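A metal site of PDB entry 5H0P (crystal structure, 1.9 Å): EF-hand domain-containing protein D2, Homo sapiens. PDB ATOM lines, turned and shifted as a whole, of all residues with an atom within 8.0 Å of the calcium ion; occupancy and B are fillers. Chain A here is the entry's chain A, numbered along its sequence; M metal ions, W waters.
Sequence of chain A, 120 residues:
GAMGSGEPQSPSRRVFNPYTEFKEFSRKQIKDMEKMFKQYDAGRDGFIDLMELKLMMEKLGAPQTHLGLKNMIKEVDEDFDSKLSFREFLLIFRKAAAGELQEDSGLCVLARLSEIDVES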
ATOM      1  N   PHE A  47       1.531   2.058   2.912  1.00  0.00           N
ATOM      2  CA  PHE A  47       0.283   2.438   3.559  1.00  0.00           C
ATOM      3  C   PHE A  47       0.503   2.739   5.008  1.00  0.00           C
ATOM      4  O   PHE A  47       1.488   2.299   5.609  1.00  0.00           O
ATOM      5  CB  PHE A  47      -0.751   1.326   3.414  1.00  0.00           C
ATOM      6  CG  PHE A  47      -1.078   1.011   1.998  1.00  0.00           C
ATOM      7  CD1 PHE A  47      -2.047   1.737   1.327  1.00  0.00           C
ATOM      8  CD2 PHE A  47      -0.389   0.012   1.319  1.00  0.00           C
ATOM      9  CE1 PHE A  47      -2.345   1.459   0.025  1.00  0.00           C
ATOM     10  CE2 PHE A  47      -0.685  -0.267   0.007  1.00  0.00           C
ATOM     11  CZ  PHE A  47      -1.656   0.450  -0.653  1.00  0.00           C
ATOM     12  N   ILE A  48      -0.413   3.527   5.577  1.00  0.00           N
ATOM     13  CA  ILE A  48      -0.477   3.634   7.006  1.00  0.00           C
ATOM     14  C   ILE A  48      -1.751   2.923   7.436  1.00  0.00           C
ATOM     15  O   ILE A  48      -2.846   3.355   7.062  1.00  0.00           O
ATOM     16  CB  ILE A  48      -0.551   5.094   7.479  1.00  0.00           C
ATOM     17  CG1 ILE A  48       0.714   5.848   7.073  1.00  0.00           C
ATOM     18  CG2 ILE A  48      -0.656   5.130   9.001  1.00  0.00           C
ATOM     19  CD1 ILE A  48       1.922   5.265   7.701  1.00  0.00           C
ATOM     20  N   ILE A  73      -9.333   7.301   9.924  1.00  0.00           N
ATOM     21  CA  ILE A  73      -9.023   6.674   8.651  1.00  0.00           C
ATOM     22  C   ILE A  73     -10.244   6.725   7.735  1.00  0.00           C
ATOM     23  O   ILE A  73     -10.119   7.101   6.579  1.00  0.00           O
ATOM     24  CB  ILE A  73      -8.511   5.232   8.871  1.00  0.00           C
ATOM     25  CG1 ILE A  73      -7.096   5.283   9.443  1.00  0.00           C
ATOM     26  CG2 ILE A  73      -8.487   4.479   7.550  1.00  0.00           C
ATOM     27  CD1 ILE A  73      -6.526   3.922   9.869  1.00  0.00           C
ATOM     28  N   VAL A  76     -11.026   9.715   5.312  1.00  0.00           N
ATOM     29  CA  VAL A  76     -10.225   9.940   4.104  1.00  0.00           C
ATOM     30  C   VAL A  76      -9.927   8.656   3.304  1.00  0.00           C
ATOM     31  O   VAL A  76      -9.143   8.681   2.361  1.00  0.00           O
ATOM     32  CB  VAL A  76      -8.899  10.687   4.406  1.00  0.00           C
ATOM     33  CG1 VAL A  76      -9.155  12.165   4.802  1.00  0.00           C
ATOM     34  CG2 VAL A  76      -8.088   9.950   5.469  1.00  0.00           C
ATOM     35  N   ASP A  77     -10.545   7.541   3.697  1.00  0.00           N
ATOM     36  CA  ASP A  77     -10.240   6.234   3.105  1.00  0.00           C
ATOM     37  C   ASP A  77     -11.140   6.015   1.890  1.00  0.00           C
ATOM     38  O   ASP A  77     -12.201   5.398   1.990  1.00  0.00           O
ATOM     39  CB  ASP A  77     -10.429   5.110   4.141  1.00  0.00           C
ATOM     40  CG  ASP A  77     -10.149   3.702   3.567  1.00  0.00           C
ATOM     41  OD1 ASP A  77      -9.318   3.565   2.671  1.00  0.00           O
ATOM     42  OD2 ASP A  77     -10.756   2.732   4.057  1.00  0.00           O
ATOM     43  N   GLU A  78     -10.695   6.538   0.755  1.00  0.00           N
ATOM     44  CA  GLU A  78     -11.479   6.500  -0.460  1.00  0.00           C
ATOM     45  C   GLU A  78     -11.546   5.150  -1.176  1.00  0.00           C
ATOM     46  O   GLU A  78     -12.412   4.972  -2.022  1.00  0.00           O
ATOM     47  CB  GLU A  78     -10.993   7.582  -1.426  1.00  0.00           C
ATOM     48  CG  GLU A  78     -11.058   8.944  -0.776  1.00  0.00           C
ATOM     49  CD  GLU A  78     -11.123  10.086  -1.769  1.00  0.00           C
ATOM     50  OE1 GLU A  78     -10.717   9.884  -2.939  1.00  0.00           O
ATOM     51  OE2 GLU A  78     -11.597  11.174  -1.377  1.00  0.00           O
ATOM     52  N   ASP A  79     -10.664   4.215  -0.834  1.00  0.00           N
ATOM     53  CA  ASP A  79     -10.715   2.914  -1.492  1.00  0.00           C
ATOM     54  C   ASP A  79     -11.005   1.786  -0.516  1.00  0.00           C
ATOM     55  O   ASP A  79     -10.776   0.622  -0.810  1.00  0.00           O
ATOM     56  CB  ASP A  79      -9.444   2.624  -2.319  1.00  0.00           C
ATOM     57  CG  ASP A  79      -8.176   2.686  -1.499  1.00  0.00           C
ATOM     58  OD1 ASP A  79      -8.237   2.679  -0.261  1.00  0.00           O
ATOM     59  OD2 ASP A  79      -7.102   2.722  -2.124  1.00  0.00           O
ATOM     60  N   PHE A  80     -11.509   2.164   0.658  1.00  0.00           N
ATOM     61  CA  PHE A  80     -12.170   1.222   1.555  1.00  0.00           C
ATOM     62  C   PHE A  80     -11.324  -0.007   1.914  1.00  0.00           C
ATOM     63  O   PHE A  80     -11.845  -1.119   2.038  1.00  0.00           O
ATOM     64  CB  PHE A  80     -13.517   0.839   0.952  1.00  0.00           C
ATOM     65  CG  PHE A  80     -14.400   2.022   0.653  1.00  0.00           C
ATOM     66  CD1 PHE A  80     -15.210   2.565   1.628  1.00  0.00           C
ATOM     67  CD2 PHE A  80     -14.371   2.632  -0.599  1.00  0.00           C
ATOM     68  CE1 PHE A  80     -16.001   3.679   1.364  1.00  0.00           C
ATOM     69  CE2 PHE A  80     -15.149   3.736  -0.870  1.00  0.00           C
ATOM     70  CZ  PHE A  80     -15.969   4.268   0.105  1.00  0.00           C
ATOM     71  N   ASP A  81     -10.013   0.194   2.061  1.00  0.00           N
ATOM     72  CA  ASP A  81      -9.157  -0.890   2.518  1.00  0.00           C
ATOM     73  C   ASP A  81      -8.703  -0.684   3.959  1.00  0.00           C
ATOM     74  O   ASP A  81      -7.814  -1.390   4.440  1.00  0.00           O
ATOM     75  CB  ASP A  81      -7.967  -1.089   1.583  1.00  0.00           C
ATOM     76  CG  ASP A  81      -7.037   0.101   1.526  1.00  0.00           C
ATOM     77  OD1 ASP A  81      -7.386   1.160   2.097  1.00  0.00           O
ATOM     78  OD2 ASP A  81      -5.960  -0.024   0.910  1.00  0.00           O
ATOM     79  N   SER A  82      -9.306   0.299   4.625  1.00  0.00           N
ATOM     80  CA  SER A  82      -9.090   0.558   6.058  1.00  0.00           C
ATOM     81  C   SER A  82      -7.654   0.961   6.379  1.00  0.00           C
ATOM     82  O   SER A  82      -7.199   0.836   7.521  1.00  0.00           O
ATOM     83  CB  SER A  82      -9.489  -0.667   6.893  1.00  0.00           C
ATOM     84  OG  SER A  82     -10.891  -0.861   6.851  1.00  0.00           O
ATOM     85  N   LYS A  83      -6.928   1.408   5.366  1.00  0.00           N
ATOM     86  CA  LYS A  83      -5.598   1.924   5.593  1.00  0.00           C
ATOM     87  C   LYS A  83      -5.386   3.125   4.675  1.00  0.00           C
ATOM     88  O   LYS A  83      -6.165   3.348   3.759  1.00  0.00           O
ATOM     89  CB  LYS A  83      -4.530   0.856   5.350  1.00  0.00           C
ATOM     90  CG  LYS A  83      -4.596   0.161   3.985  1.00  0.00           C
ATOM     91  CD  LYS A  83      -3.512  -0.905   3.827  1.00  0.00           C
ATOM     92  CE  LYS A  83      -3.590  -1.571   2.456  1.00  0.00           C
ATOM     93  NZ  LYS A  83      -2.489  -2.530   2.258  1.00  0.00           N
ATOM     94  N   LEU A  84      -4.342   3.899   4.943  1.00  0.00           N
ATOM     95  CA  LEU A  84      -4.136   5.144   4.213  1.00  0.00           C
ATOM     96  C   LEU A  84      -3.005   5.044   3.215  1.00  0.00           C
ATOM     97  O   LEU A  84      -1.872   4.757   3.590  1.00  0.00           O
ATOM     98  CB  LEU A  84      -3.780   6.275   5.203  1.00  0.00           C
ATOM     99  CG  LEU A  84      -4.706   6.612   6.364  1.00  0.00           C
ATOM    100  CD1 LEU A  84      -4.069   7.715   7.215  1.00  0.00           C
ATOM    101  CD2 LEU A  84      -6.058   7.061   5.869  1.00  0.00           C
ATOM    102  N   SER A  85      -3.322   5.326   1.958  1.00  0.00           N
ATOM    103  CA  SER A  85      -2.297   5.530   0.936  1.00  0.00           C
ATOM    104  C   SER A  85      -1.737   6.940   1.072  1.00  0.00           C
ATOM    105  O   SER A  85      -2.289   7.765   1.817  1.00  0.00           O
ATOM    106  CB  SER A  85      -2.897   5.371  -0.456  1.00  0.00           C
ATOM    107  OG  SER A  85      -3.773   6.447  -0.731  1.00  0.00           O
ATOM    108  N   PHE A  86      -0.660   7.246   0.345  1.00  0.00           N
ATOM    109  CA  PHE A  86      -0.080   8.575   0.463  1.00  0.00           C
ATOM    110  C   PHE A  86      -1.070   9.636  -0.026  1.00  0.00           C
ATOM    111  O   PHE A  86      -1.168  10.723   0.547  1.00  0.00           O
ATOM    112  CB  PHE A  86       1.254   8.673  -0.285  1.00  0.00           C
ATOM    113  CG  PHE A  86       1.874  10.046  -0.237  1.00  0.00           C
ATOM    114  CD1 PHE A  86       1.907  10.757   0.957  1.00  0.00           C
ATOM    115  CD2 PHE A  86       2.395  10.634  -1.375  1.00  0.00           C
ATOM    116  CE1 PHE A  86       2.453  12.025   1.014  1.00  0.00           C
ATOM    117  CE2 PHE A  86       2.952  11.902  -1.326  1.00  0.00           C
ATOM    118  CZ  PHE A  86       2.987  12.593  -0.130  1.00  0.00           C
ATOM    119  N   GLU A  88      -4.289   9.538   0.251  1.00  0.00           N
ATOM    120  CA  GLU A  88      -5.301   9.720   1.282  1.00  0.00           C
ATOM    121  C   GLU A  88      -4.724  10.499   2.475  1.00  0.00           C
ATOM    122  O   GLU A  88      -5.457  11.240   3.135  1.00  0.00           O
ATOM    123  CB  GLU A  88      -5.906   8.370   1.724  1.00  0.00           C
ATOM    124  CG  GLU A  88      -6.754   7.668   0.646  1.00  0.00           C
ATOM    125  CD  GLU A  88      -6.956   6.177   0.954  1.00  0.00           C
ATOM    126  OE1 GLU A  88      -6.185   5.650   1.781  1.00  0.00           O
ATOM    127  OE2 GLU A  88      -7.867   5.525   0.380  1.00  0.00           O
ATOM    128  N   PHE A  89      -3.430  10.349   2.731  1.00  0.00           N
ATOM    129  CA  PHE A  89      -2.730  11.115   3.755  1.00  0.00           C
ATOM    130  C   PHE A  89      -2.782  12.581   3.392  1.00  0.00           C
ATOM    131  O   PHE A  89      -3.086  13.434   4.220  1.00  0.00           O
ATOM    132  CB  PHE A  89      -1.270  10.683   3.849  1.00  0.00           C
ATOM    133  CG  PHE A  89      -0.539  11.193   5.061  1.00  0.00           C
ATOM    134  CD1 PHE A  89      -0.944  10.834   6.347  1.00  0.00           C
ATOM    135  CD2 PHE A  89       0.561  12.010   4.924  1.00  0.00           C
ATOM    136  CE1 PHE A  89      -0.243  11.299   7.467  1.00  0.00           C
ATOM    137  CE2 PHE A  89       1.263  12.473   6.034  1.00  0.00           C
ATOM    138  CZ  PHE A  89       0.850  12.123   7.308  1.00  0.00           C
HETATM  139 CA    CA M   1      -7.255   3.447   1.653  1.00  0.00          CA
HETATM  140  O   HOH W   1      -5.307   2.645   0.488  1.00  0.00           O
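OD2 of Asp 77 is in hydrogen-bond range of N of Ser 82 (2.9 Å).
The backbone NH (N) of Phe 80 sits close to the side-chain carboxylate (OD1) of Asp 77, at 3.3 Å.
N of Glu 88 is in hydrogen-bond range of OG of Ser 85 (3.3 Å).
The side-chain carboxylate (OE2) of Glu 88 lies close to the backbone NH (N) of Glu 78 (3.0 Å).
Within 4 Å of the calcium ion: Asp 77, Asp 79, Asp 81, Lys 83 and Glu 88.
The nearest printed residue that does not touch the calcium ion is Ser 85 (4.4 Å).
OD1 of Asp 79 is bound to the calcium ion (2.3 Å).
The calcium ion is bound by the side-chain carboxylate (OD1) of Asp 77 (2.3 Å).
The calcium ion is bound by OD1 of Asp 81 (2.3 Å).
The backbone carbonyl oxygen (O) of Lys 83 is bound to the calcium ion, 2.4 Å away.
The calcium ion is bound by water W1 (2.4 Å).
OE1 of Glu 88 binds the calcium ion.
The side-chain carboxylate (OE2) of Glu 88 is bound to the calcium ion (2.5 Å).
The calcium ion has seven donor atoms within binding distance.
Water W1 bridges the side-chain carboxylate of Asp 81 (2.8 Å) and the side-chain carboxylate of Asp 79 (3.2 Å).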
